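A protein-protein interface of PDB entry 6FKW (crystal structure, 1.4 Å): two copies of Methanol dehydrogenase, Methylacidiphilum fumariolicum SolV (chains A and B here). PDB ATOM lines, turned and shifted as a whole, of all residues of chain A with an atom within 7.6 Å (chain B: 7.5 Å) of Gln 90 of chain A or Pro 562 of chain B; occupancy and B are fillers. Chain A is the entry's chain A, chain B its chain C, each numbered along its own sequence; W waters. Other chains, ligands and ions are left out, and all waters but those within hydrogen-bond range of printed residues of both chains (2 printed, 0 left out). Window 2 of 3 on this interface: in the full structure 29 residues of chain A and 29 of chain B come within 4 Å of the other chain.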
ATOM      1  N   PHE A  46      -7.602  26.367  13.288  1.00  0.00           N
ATOM      2  CA  PHE A  46      -6.888  25.116  13.058  1.00  0.00           C
ATOM      3  C   PHE A  46      -6.662  24.435  14.400  1.00  0.00           C
ATOM      4  O   PHE A  46      -6.076  25.027  15.301  1.00  0.00           O
ATOM      5  CB  PHE A  46      -5.553  25.393  12.366  1.00  0.00           C
ATOM      6  CG  PHE A  46      -4.664  24.190  12.262  1.00  0.00           C
ATOM      7  CD1 PHE A  46      -4.965  23.157  11.388  1.00  0.00           C
ATOM      8  CD2 PHE A  46      -3.530  24.089  13.050  1.00  0.00           C
ATOM      9  CE1 PHE A  46      -4.141  22.045  11.301  1.00  0.00           C
ATOM     10  CE2 PHE A  46      -2.703  22.983  12.966  1.00  0.00           C
ATOM     11  CZ  PHE A  46      -3.013  21.963  12.090  1.00  0.00           C
ATOM     12  N   THR A  48      -4.868  22.019  16.963  1.00  0.00           N
ATOM     13  CA  THR A  48      -3.503  21.517  17.116  1.00  0.00           C
ATOM     14  C   THR A  48      -3.453  20.015  17.374  1.00  0.00           C
ATOM     15  O   THR A  48      -2.379  19.420  17.293  1.00  0.00           O
ATOM     16  CB  THR A  48      -2.779  22.198  18.280  1.00  0.00           C
ATOM     17  OG1 THR A  48      -3.429  21.835  19.507  1.00  0.00           O
ATOM     18  CG2 THR A  48      -2.783  23.716  18.112  1.00  0.00           C
ATOM     19  N   HIS A  74       3.147  17.948  18.499  1.00  0.00           N
ATOM     20  CA  HIS A  74       2.824  17.953  17.072  1.00  0.00           C
ATOM     21  C   HIS A  74       3.329  19.246  16.447  1.00  0.00           C
ATOM     22  O   HIS A  74       3.209  20.315  17.043  1.00  0.00           O
ATOM     23  CB  HIS A  74       1.315  17.886  16.835  1.00  0.00           C
ATOM     24  CG  HIS A  74       0.641  16.712  17.472  1.00  0.00           C
ATOM     25  ND1 HIS A  74       0.893  15.410  17.099  1.00  0.00           N
ATOM     26  CD2 HIS A  74      -0.285  16.649  18.457  1.00  0.00           C
ATOM     27  CE1 HIS A  74       0.153  14.595  17.829  1.00  0.00           C
ATOM     28  NE2 HIS A  74      -0.571  15.322  18.660  1.00  0.00           N
ATOM     29  N   VAL A  75       3.892  19.138  15.247  1.00  0.00           N
ATOM     30  CA  VAL A  75       4.333  20.301  14.483  1.00  0.00           C
ATOM     31  C   VAL A  75       3.685  20.255  13.104  1.00  0.00           C
ATOM     32  O   VAL A  75       3.616  19.201  12.473  1.00  0.00           O
ATOM     33  CB  VAL A  75       5.872  20.347  14.360  1.00  0.00           C
ATOM     34  CG1 VAL A  75       6.308  21.492  13.455  1.00  0.00           C
ATOM     35  CG2 VAL A  75       6.490  20.486  15.743  1.00  0.00           C
ATOM     36  N   TYR A  76       3.206  21.409  12.646  1.00  0.00           N
ATOM     37  CA  TYR A  76       2.522  21.512  11.365  1.00  0.00           C
ATOM     38  C   TYR A  76       3.058  22.690  10.579  1.00  0.00           C
ATOM     39  O   TYR A  76       3.402  23.723  11.157  1.00  0.00           O
ATOM     40  CB  TYR A  76       1.027  21.746  11.568  1.00  0.00           C
ATOM     41  CG  TYR A  76       0.362  20.783  12.515  1.00  0.00           C
ATOM     42  CD1 TYR A  76      -0.142  19.569  12.064  1.00  0.00           C
ATOM     43  CD2 TYR A  76       0.229  21.095  13.865  1.00  0.00           C
ATOM     44  CE1 TYR A  76      -0.758  18.690  12.936  1.00  0.00           C
ATOM     45  CE2 TYR A  76      -0.388  20.220  14.747  1.00  0.00           C
ATOM     46  CZ  TYR A  76      -0.878  19.022  14.274  1.00  0.00           C
ATOM     47  OH  TYR A  76      -1.490  18.143  15.137  1.00  0.00           O
ATOM     48  N   ALA A  77       3.118  22.515   9.264  1.00  0.00           N
ATOM     49  CA  ALA A  77       3.327  23.614   8.336  1.00  0.00           C
ATOM     50  C   ALA A  77       2.032  23.802   7.565  1.00  0.00           C
ATOM     51  O   ALA A  77       1.519  22.853   6.959  1.00  0.00           O
ATOM     52  CB  ALA A  77       4.470  23.311   7.388  1.00  0.00           C
ATOM     53  N   ILE A  87      -2.809  21.897   5.015  1.00  0.00           N
ATOM     54  CA  ILE A  87      -1.725  21.315   5.788  1.00  0.00           C
ATOM     55  C   ILE A  87      -0.666  20.820   4.806  1.00  0.00           C
ATOM     56  O   ILE A  87      -0.900  19.876   4.048  1.00  0.00           O
ATOM     57  CB  ILE A  87      -2.182  20.153   6.691  1.00  0.00           C
ATOM     58  CG1 ILE A  87      -3.323  20.595   7.615  1.00  0.00           C
ATOM     59  CG2 ILE A  87      -0.995  19.648   7.505  1.00  0.00           C
ATOM     60  CD1 ILE A  87      -3.961  19.457   8.386  1.00  0.00           C
ATOM     61  N   LYS A  88       0.490  21.470   4.827  1.00  0.00           N
ATOM     62  CA  LYS A  88       1.586  21.147   3.928  1.00  0.00           C
ATOM     63  C   LYS A  88       2.329  19.904   4.403  1.00  0.00           C
ATOM     64  O   LYS A  88       2.630  19.005   3.617  1.00  0.00           O
ATOM     65  CB  LYS A  88       2.545  22.332   3.840  1.00  0.00           C
ATOM     66  CG  LYS A  88       3.641  22.159   2.809  1.00  0.00           C
ATOM     67  CD  LYS A  88       4.443  23.437   2.646  1.00  0.00           C
ATOM     68  CE  LYS A  88       5.439  23.312   1.511  1.00  0.00           C
ATOM     69  NZ  LYS A  88       6.191  24.575   1.288  1.00  0.00           N
ATOM     70  N   TRP A  89       2.627  19.869   5.697  1.00  0.00           N
ATOM     71  CA  TRP A  89       3.189  18.672   6.311  1.00  0.00           C
ATOM     72  C   TRP A  89       2.940  18.673   7.804  1.00  0.00           C
ATOM     73  O   TRP A  89       2.570  19.693   8.385  1.00  0.00           O
ATOM     74  CB  TRP A  89       4.688  18.506   5.995  1.00  0.00           C
ATOM     75  CG  TRP A  89       5.617  19.651   6.352  1.00  0.00           C
ATOM     76  CD1 TRP A  89       6.117  20.591   5.493  1.00  0.00           C
ATOM     77  CD2 TRP A  89       6.163  19.964   7.645  1.00  0.00           C
ATOM     78  NE1 TRP A  89       6.932  21.464   6.170  1.00  0.00           N
ATOM     79  CE2 TRP A  89       6.979  21.104   7.490  1.00  0.00           C
ATOM     80  CE3 TRP A  89       6.042  19.393   8.917  1.00  0.00           C
ATOM     81  CZ2 TRP A  89       7.670  21.685   8.557  1.00  0.00           C
ATOM     82  CZ3 TRP A  89       6.728  19.971   9.975  1.00  0.00           C
ATOM     83  CH2 TRP A  89       7.531  21.105   9.790  1.00  0.00           C
ATOM     84  N   GLN A  90       3.137  17.512   8.419  1.00  0.00           N
ATOM     85  CA  GLN A  90       3.094  17.417   9.867  1.00  0.00           C
ATOM     86  C   GLN A  90       4.144  16.448  10.370  1.00  0.00           C
ATOM     87  O   GLN A  90       4.563  15.530   9.657  1.00  0.00           O
ATOM     88  CB  GLN A  90       1.707  17.039  10.372  1.00  0.00           C
ATOM     89  CG  GLN A  90       1.202  15.671   9.981  1.00  0.00           C
ATOM     90  CD  GLN A  90      -0.065  15.326  10.734  1.00  0.00           C
ATOM     91  OE1 GLN A  90      -0.017  14.844  11.870  1.00  0.00           O
ATOM     92  NE2 GLN A  90      -1.210  15.573  10.108  1.00  0.00           N
ATOM     93  N   TYR A  91       4.567  16.673  11.604  1.00  0.00           N
ATOM     94  CA  TYR A  91       5.580  15.849  12.235  1.00  0.00           C
ATOM     95  C   TYR A  91       5.260  15.708  13.705  1.00  0.00           C
ATOM     96  O   TYR A  91       4.934  16.692  14.367  1.00  0.00           O
ATOM     97  CB  TYR A  91       6.957  16.487  12.082  1.00  0.00           C
ATOM     98  CG  TYR A  91       8.055  15.752  12.822  1.00  0.00           C
ATOM     99  CD1 TYR A  91       8.669  14.641  12.260  1.00  0.00           C
ATOM    100  CD2 TYR A  91       8.477  16.168  14.082  1.00  0.00           C
ATOM    101  CE1 TYR A  91       9.673  13.965  12.932  1.00  0.00           C
ATOM    102  CE2 TYR A  91       9.479  15.498  14.762  1.00  0.00           C
ATOM    103  CZ  TYR A  91      10.074  14.402  14.183  1.00  0.00           C
ATOM    104  OH  TYR A  91      11.074  13.720  14.842  1.00  0.00           O
ATOM    105  N   THR A  92       5.351  14.481  14.209  1.00  0.00           N
ATOM    106  CA  THR A  92       5.246  14.238  15.638  1.00  0.00           C
ATOM    107  C   THR A  92       6.411  13.348  16.058  1.00  0.00           C
ATOM    108  O   THR A  92       6.553  12.242  15.541  1.00  0.00           O
ATOM    109  CB  THR A  92       3.920  13.561  16.018  1.00  0.00           C
ATOM    110  OG1 THR A  92       2.821  14.340  15.525  1.00  0.00           O
ATOM    111  CG2 THR A  92       3.801  13.433  17.536  1.00  0.00           C
ATOM    112  N   LEU A 131      14.000  19.850  11.318  1.00  0.00           N
ATOM    113  CA  LEU A 131      13.133  19.379  10.248  1.00  0.00           C
ATOM    114  C   LEU A 131      13.371  20.242   9.019  1.00  0.00           C
ATOM    115  O   LEU A 131      13.683  21.424   9.146  1.00  0.00           O
ATOM    116  CB  LEU A 131      11.667  19.521  10.653  1.00  0.00           C
ATOM    117  CG  LEU A 131      11.236  18.863  11.958  1.00  0.00           C
ATOM    118  CD1 LEU A 131       9.776  19.188  12.253  1.00  0.00           C
ATOM    119  CD2 LEU A 131      11.464  17.362  11.913  1.00  0.00           C
ATOM    120  N   THR A 135       9.448  20.241   3.623  1.00  0.00           N
ATOM    121  CA  THR A 135       8.887  18.887   3.545  1.00  0.00           C
ATOM    122  C   THR A 135       8.517  18.255   4.887  1.00  0.00           C
ATOM    123  O   THR A 135       7.762  17.288   4.917  1.00  0.00           O
ATOM    124  CB  THR A 135       9.873  17.929   2.863  1.00  0.00           C
ATOM    125  OG1 THR A 135      11.018  17.762   3.703  1.00  0.00           O
ATOM    126  CG2 THR A 135      10.305  18.466   1.504  1.00  0.00           C
ATOM    127  N   GLY A 136       9.048  18.783   5.987  1.00  0.00           N
ATOM    128  CA  GLY A 136       8.830  18.195   7.303  1.00  0.00           C
ATOM    129  C   GLY A 136       9.712  17.001   7.612  1.00  0.00           C
ATOM    130  O   GLY A 136       9.560  16.391   8.672  1.00  0.00           O
ATOM    131  N   LYS A 137      10.629  16.669   6.698  1.00  0.00           N
ATOM    132  CA  LYS A 137      11.529  15.531   6.882  1.00  0.00           C
ATOM    133  C   LYS A 137      12.492  15.813   8.025  1.00  0.00           C
ATOM    134  O   LYS A 137      13.072  16.890   8.116  1.00  0.00           O
ATOM    135  CB  LYS A 137      12.323  15.237   5.604  1.00  0.00           C
ATOM    136  CG  LYS A 137      13.106  13.931   5.646  1.00  0.00           C
ATOM    137  CD  LYS A 137      14.116  13.830   4.512  1.00  0.00           C
ATOM    138  CE  LYS A 137      14.766  12.454   4.481  1.00  0.00           C
ATOM    139  NZ  LYS A 137      15.919  12.385   3.541  1.00  0.00           N
ATOM    140  N   PHE B 464     -14.871  14.880   0.261  1.00  0.00           N
ATOM    141  CA  PHE B 464     -15.015  13.871   1.304  1.00  0.00           C
ATOM    142  C   PHE B 464     -16.479  13.506   1.516  1.00  0.00           C
ATOM    143  O   PHE B 464     -17.374  14.282   1.165  1.00  0.00           O
ATOM    144  CB  PHE B 464     -14.407  14.374   2.618  1.00  0.00           C
ATOM    145  CG  PHE B 464     -12.929  14.615   2.540  1.00  0.00           C
ATOM    146  CD1 PHE B 464     -12.047  13.547   2.469  1.00  0.00           C
ATOM    147  CD2 PHE B 464     -12.416  15.903   2.534  1.00  0.00           C
ATOM    148  CE1 PHE B 464     -10.681  13.757   2.393  1.00  0.00           C
ATOM    149  CE2 PHE B 464     -11.046  16.120   2.457  1.00  0.00           C
ATOM    150  CZ  PHE B 464     -10.179  15.042   2.390  1.00  0.00           C
ATOM    151  N   PHE B 533     -15.471   6.883   8.914  1.00  0.00           N
ATOM    152  CA  PHE B 533     -14.590   7.338   7.827  1.00  0.00           C
ATOM    153  C   PHE B 533     -13.354   8.073   8.358  1.00  0.00           C
ATOM    154  O   PHE B 533     -12.286   8.009   7.744  1.00  0.00           O
ATOM    155  CB  PHE B 533     -15.328   8.215   6.814  1.00  0.00           C
ATOM    156  CG  PHE B 533     -14.509   8.534   5.588  1.00  0.00           C
ATOM    157  CD1 PHE B 533     -14.471   7.661   4.511  1.00  0.00           C
ATOM    158  CD2 PHE B 533     -13.765   9.712   5.513  1.00  0.00           C
ATOM    159  CE1 PHE B 533     -13.716   7.952   3.385  1.00  0.00           C
ATOM    160  CE2 PHE B 533     -13.012  10.003   4.389  1.00  0.00           C
ATOM    161  CZ  PHE B 533     -12.988   9.125   3.327  1.00  0.00           C
ATOM    162  N   ALA B 536      -9.018   6.631  10.765  1.00  0.00           N
ATOM    163  CA  ALA B 536      -7.575   6.706  10.530  1.00  0.00           C
ATOM    164  C   ALA B 536      -6.959   7.932  11.215  1.00  0.00           C
ATOM    165  O   ALA B 536      -5.833   7.883  11.709  1.00  0.00           O
ATOM    166  CB  ALA B 536      -7.277   6.728   9.038  1.00  0.00           C
ATOM    167  N   VAL B 537      -7.705   9.031  11.245  1.00  0.00           N
ATOM    168  CA  VAL B 537      -7.238  10.251  11.896  1.00  0.00           C
ATOM    169  C   VAL B 537      -7.499  10.188  13.404  1.00  0.00           C
ATOM    170  O   VAL B 537      -6.600  10.436  14.198  1.00  0.00           O
ATOM    171  CB  VAL B 537      -7.903  11.498  11.281  1.00  0.00           C
ATOM    172  CG1 VAL B 537      -7.472  12.763  12.014  1.00  0.00           C
ATOM    173  CG2 VAL B 537      -7.564  11.591   9.797  1.00  0.00           C
ATOM    174  N   ASN B 540      -5.240   7.577  14.817  1.00  0.00           N
ATOM    175  CA  ASN B 540      -3.857   7.685  14.339  1.00  0.00           C
ATOM    176  C   ASN B 540      -3.347   6.376  13.739  1.00  0.00           C
ATOM    177  O   ASN B 540      -2.323   5.833  14.169  1.00  0.00           O
ATOM    178  CB  ASN B 540      -2.930   8.164  15.468  1.00  0.00           C
ATOM    179  CG  ASN B 540      -1.590   8.677  14.953  1.00  0.00           C
ATOM    180  OD1 ASN B 540      -1.476   9.118  13.808  1.00  0.00           O
ATOM    181  ND2 ASN B 540      -0.570   8.621  15.801  1.00  0.00           N
ATOM    182  N   LEU B 541      -4.070   5.874  12.742  1.00  0.00           N
ATOM    183  CA  LEU B 541      -3.730   4.609  12.098  1.00  0.00           C
ATOM    184  C   LEU B 541      -2.900   4.853  10.847  1.00  0.00           C
ATOM    185  O   LEU B 541      -3.155   5.800  10.102  1.00  0.00           O
ATOM    186  CB  LEU B 541      -4.990   3.826  11.737  1.00  0.00           C
ATOM    187  CG  LEU B 541      -5.917   3.498  12.906  1.00  0.00           C
ATOM    188  CD1 LEU B 541      -7.231   2.932  12.394  1.00  0.00           C
ATOM    189  CD2 LEU B 541      -5.246   2.536  13.876  1.00  0.00           C
ATOM    190  N   PRO B 543      -1.147   4.025   7.006  1.00  0.00           N
ATOM    191  CA  PRO B 543      -1.681   3.599   5.709  1.00  0.00           C
ATOM    192  C   PRO B 543      -1.289   2.178   5.286  1.00  0.00           C
ATOM    193  O   PRO B 543      -1.832   1.668   4.306  1.00  0.00           O
ATOM    194  CB  PRO B 543      -1.056   4.603   4.743  1.00  0.00           C
ATOM    195  CG  PRO B 543       0.254   4.936   5.366  1.00  0.00           C
ATOM    196  CD  PRO B 543       0.021   4.912   6.852  1.00  0.00           C
ATOM    197  N   VAL B 553      -9.569   2.633   6.611  1.00  0.00           N
ATOM    198  CA  VAL B 553      -8.216   3.185   6.564  1.00  0.00           C
ATOM    199  C   VAL B 553      -7.786   3.454   5.122  1.00  0.00           C
ATOM    200  O   VAL B 553      -7.386   4.568   4.794  1.00  0.00           O
ATOM    201  CB  VAL B 553      -7.196   2.289   7.295  1.00  0.00           C
ATOM    202  CG1 VAL B 553      -5.770   2.765   7.043  1.00  0.00           C
ATOM    203  CG2 VAL B 553      -7.494   2.285   8.788  1.00  0.00           C
ATOM    204  N   VAL B 555      -9.497   3.798   2.285  1.00  0.00           N
ATOM    205  CA  VAL B 555     -10.263   4.819   1.567  1.00  0.00           C
ATOM    206  C   VAL B 555      -9.988   6.239   2.083  1.00  0.00           C
ATOM    207  O   VAL B 555      -9.927   7.183   1.291  1.00  0.00           O
ATOM    208  CB  VAL B 555     -11.779   4.497   1.544  1.00  0.00           C
ATOM    209  CG1 VAL B 555     -12.401   4.586   2.932  1.00  0.00           C
ATOM    210  CG2 VAL B 555     -12.506   5.392   0.550  1.00  0.00           C
ATOM    211  N   ALA B 556      -9.819   6.392   3.397  1.00  0.00           N
ATOM    212  CA  ALA B 556      -9.499   7.696   3.978  1.00  0.00           C
ATOM    213  C   ALA B 556      -8.161   8.225   3.459  1.00  0.00           C
ATOM    214  O   ALA B 556      -8.046   9.404   3.125  1.00  0.00           O
ATOM    215  CB  ALA B 556      -9.498   7.619   5.501  1.00  0.00           C
ATOM    216  N   TYR B 557      -7.152   7.357   3.388  1.00  0.00           N
ATOM    217  CA  TYR B 557      -5.855   7.751   2.825  1.00  0.00           C
ATOM    218  C   TYR B 557      -5.943   8.055   1.326  1.00  0.00           C
ATOM    219  O   TYR B 557      -5.337   9.022   0.861  1.00  0.00           O
ATOM    220  CB  TYR B 557      -4.776   6.698   3.106  1.00  0.00           C
ATOM    221  CG  TYR B 557      -4.104   6.867   4.450  1.00  0.00           C
ATOM    222  CD1 TYR B 557      -3.077   7.792   4.627  1.00  0.00           C
ATOM    223  CD2 TYR B 557      -4.490   6.104   5.545  1.00  0.00           C
ATOM    224  CE1 TYR B 557      -2.457   7.951   5.858  1.00  0.00           C
ATOM    225  CE2 TYR B 557      -3.879   6.254   6.778  1.00  0.00           C
ATOM    226  CZ  TYR B 557      -2.865   7.175   6.931  1.00  0.00           C
ATOM    227  OH  TYR B 557      -2.261   7.319   8.158  1.00  0.00           O
ATOM    228  N   GLN B 558      -6.693   7.246   0.574  1.00  0.00           N
ATOM    229  CA  GLN B 558      -6.914   7.515  -0.856  1.00  0.00           C
ATOM    230  C   GLN B 558      -7.571   8.877  -1.073  1.00  0.00           C
ATOM    231  O   GLN B 558      -7.196   9.615  -1.981  1.00  0.00           O
ATOM    232  CB  GLN B 558      -7.776   6.425  -1.502  1.00  0.00           C
ATOM    233  CG  GLN B 558      -7.048   5.113  -1.729  1.00  0.00           C
ATOM    234  CD  GLN B 558      -7.968   3.981  -2.153  1.00  0.00           C
ATOM    235  OE1 GLN B 558      -9.193   4.121  -2.167  1.00  0.00           O
ATOM    236  NE2 GLN B 558      -7.375   2.845  -2.499  1.00  0.00           N
ATOM    237  N   ALA B 559      -8.548   9.198  -0.230  1.00  0.00           N
ATOM    238  CA  ALA B 559      -9.249  10.481  -0.298  1.00  0.00           C
ATOM    239  C   ALA B 559      -8.401  11.650   0.218  1.00  0.00           C
ATOM    240  O   ALA B 559      -8.705  12.807  -0.068  1.00  0.00           O
ATOM    241  CB  ALA B 559     -10.555  10.403   0.483  1.00  0.00           C
ATOM    242  N   GLY B 560      -7.351  11.347   0.976  1.00  0.00           N
ATOM    243  CA  GLY B 560      -6.443  12.361   1.504  1.00  0.00           C
ATOM    244  C   GLY B 560      -6.885  12.970   2.825  1.00  0.00           C
ATOM    245  O   GLY B 560      -6.466  14.077   3.165  1.00  0.00           O
ATOM    246  N   LEU B 561      -7.717  12.259   3.582  1.00  0.00           N
ATOM    247  CA  LEU B 561      -8.242  12.812   4.840  1.00  0.00           C
ATOM    248  C   LEU B 561      -7.130  13.104   5.855  1.00  0.00           C
ATOM    249  O   LEU B 561      -7.129  14.169   6.461  1.00  0.00           O
ATOM    250  CB  LEU B 561      -9.332  11.921   5.460  1.00  0.00           C
ATOM    251  CG  LEU B 561     -10.048  12.547   6.664  1.00  0.00           C
ATOM    252  CD1 LEU B 561     -10.950  13.694   6.231  1.00  0.00           C
ATOM    253  CD2 LEU B 561     -10.855  11.505   7.429  1.00  0.00           C
ATOM    254  N   PRO B 562      -6.178  12.166   6.046  1.00  0.00           N
ATOM    255  CA  PRO B 562      -5.097  12.463   6.994  1.00  0.00           C
ATOM    256  C   PRO B 562      -4.250  13.696   6.662  1.00  0.00           C
ATOM    257  O   PRO B 562      -3.665  14.285   7.569  1.00  0.00           O
ATOM    258  CB  PRO B 562      -4.256  11.183   6.973  1.00  0.00           C
ATOM    259  CG  PRO B 562      -5.237  10.124   6.600  1.00  0.00           C
ATOM    260  CD  PRO B 562      -6.085  10.783   5.551  1.00  0.00           C
ATOM    261  N   LYS B 563      -4.188  14.080   5.386  1.00  0.00           N
ATOM    262  CA  LYS B 563      -3.526  15.322   4.982  1.00  0.00           C
ATOM    263  C   LYS B 563      -4.429  16.549   5.097  1.00  0.00           C
ATOM    264  O   LYS B 563      -3.952  17.676   4.961  1.00  0.00           O
ATOM    265  CB  LYS B 563      -3.061  15.236   3.529  1.00  0.00           C
ATOM    266  CG  LYS B 563      -2.161  14.054   3.205  1.00  0.00           C
ATOM    267  CD  LYS B 563      -1.494  14.214   1.841  1.00  0.00           C
ATOM    268  CE  LYS B 563      -2.487  14.590   0.744  1.00  0.00           C
ATOM    269  NZ  LYS B 563      -1.877  14.567  -0.616  1.00  0.00           N
ATOM    270  N   ALA B 564      -5.722  16.334   5.338  1.00  0.00           N
ATOM    271  CA  ALA B 564      -6.721  17.409   5.287  1.00  0.00           C
ATOM    272  C   ALA B 564      -7.178  17.909   6.657  1.00  0.00           C
ATOM    273  O   ALA B 564      -7.706  19.016   6.765  1.00  0.00           O
ATOM    274  CB  ALA B 564      -7.932  16.947   4.492  1.00  0.00           C
ATOM    275  N   THR B 565      -6.990  17.110   7.704  1.00  0.00           N
ATOM    276  CA  THR B 565      -7.542  17.474   9.001  1.00  0.00           C
ATOM    277  C   THR B 565      -6.796  16.848  10.174  1.00  0.00           C
ATOM    278  O   THR B 565      -6.211  15.773  10.054  1.00  0.00           O
ATOM    279  CB  THR B 565      -9.039  17.097   9.088  1.00  0.00           C
ATOM    280  OG1 THR B 565      -9.586  17.562  10.330  1.00  0.00           O
ATOM    281  CG2 THR B 565      -9.243  15.591   8.965  1.00  0.00           C
ATOM    282  N   THR B 566      -6.843  17.552  11.302  1.00  0.00           N
ATOM    283  CA  THR B 566      -6.348  17.073  12.583  1.00  0.00           C
ATOM    284  C   THR B 566      -7.546  16.791  13.481  1.00  0.00           C
ATOM    285  O   THR B 566      -8.671  17.168  13.154  1.00  0.00           O
ATOM    286  CB  THR B 566      -5.496  18.154  13.264  1.00  0.00           C
ATOM    287  OG1 THR B 566      -6.245  19.378  13.308  1.00  0.00           O
ATOM    288  CG2 THR B 566      -4.201  18.376  12.497  1.00  0.00           C
HETATM  289  O   HOH W   1      -3.896  14.451  10.672  1.00  0.00           O
HETATM  290  O   HOH W   2      -4.996  20.355   4.267  1.00  0.00           O
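O of Thr 48 of chain A is in hydrogen-bond range of OH of Tyr 76 of chain A, at 2.7 Å.
Water W1 lies within hydrogen-bond range of the backbone carbonyl oxygen (O) of Thr 565 of chain B, the side-chain amide nitrogen (NE2) of Gln 90 of chain A and the backbone carbonyl oxygen (O) of Pro 562 of chain B.
Water W2 lies within hydrogen-bond range of the backbone NH (N) of Ile 87 of chain A (2.8 Å) and the backbone carbonyl oxygen (O) of Lys 563 of chain B (3.0 Å).
Among the printed residues, merely in contact across the chains: Phe 46 of chain A with Thr 566 of chain B (3.8 Å), Tyr 76 of chain A with Thr 566 of chain B (3.5 Å), Ile 87 of chain A with Lys 563 of chain B (3.5 Å), Ile 87 of chain A with Ala 564 of chain B (3.97 Å), Ile 87 of chain A with Thr 565 of chain B (3.9 Å) and Gln 90 of chain A with Pro 562 of chain B (3.8 Å).
No position is printed for both chains.
Of the 6 pairs that touch across the chains among the printed residues, none has its exchanged pair printed and touching as well.
Of the 20 printed residues of chain B, 5 touch a printed residue of chain A.
Of the 16 printed residues of chain A, 4 touch a printed residue of chain B.
Hydrophobic or aromatic side chains of chain A that line the printed part of chain B: Phe 46, Tyr 76 and Ile 87.
Of the printed residues of chain B, Gln 90 of chain A touches Pro 562.
Pro 562 of chain B touches just one residue of chain A: Gln 90 (3.8 Å).
Of the printed residues of chain A, Ala 564 of chain B touches Ile 87.
Printed residues of chain A within 4 Å of Thr 565 of chain B: Ile 87 (3.9 Å).
Of the printed residues of chain A, Lys 563 of chain B touches Ile 87 (3.5 Å).
Thr 48 of chain A touches none of the printed residues of chain B.
Lys 88 of chain A touches none of the printed residues of chain B.
The nearest residue of chain A that does not touch Pro 562 of chain B is Ile 87 of chain A (5.2 Å).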
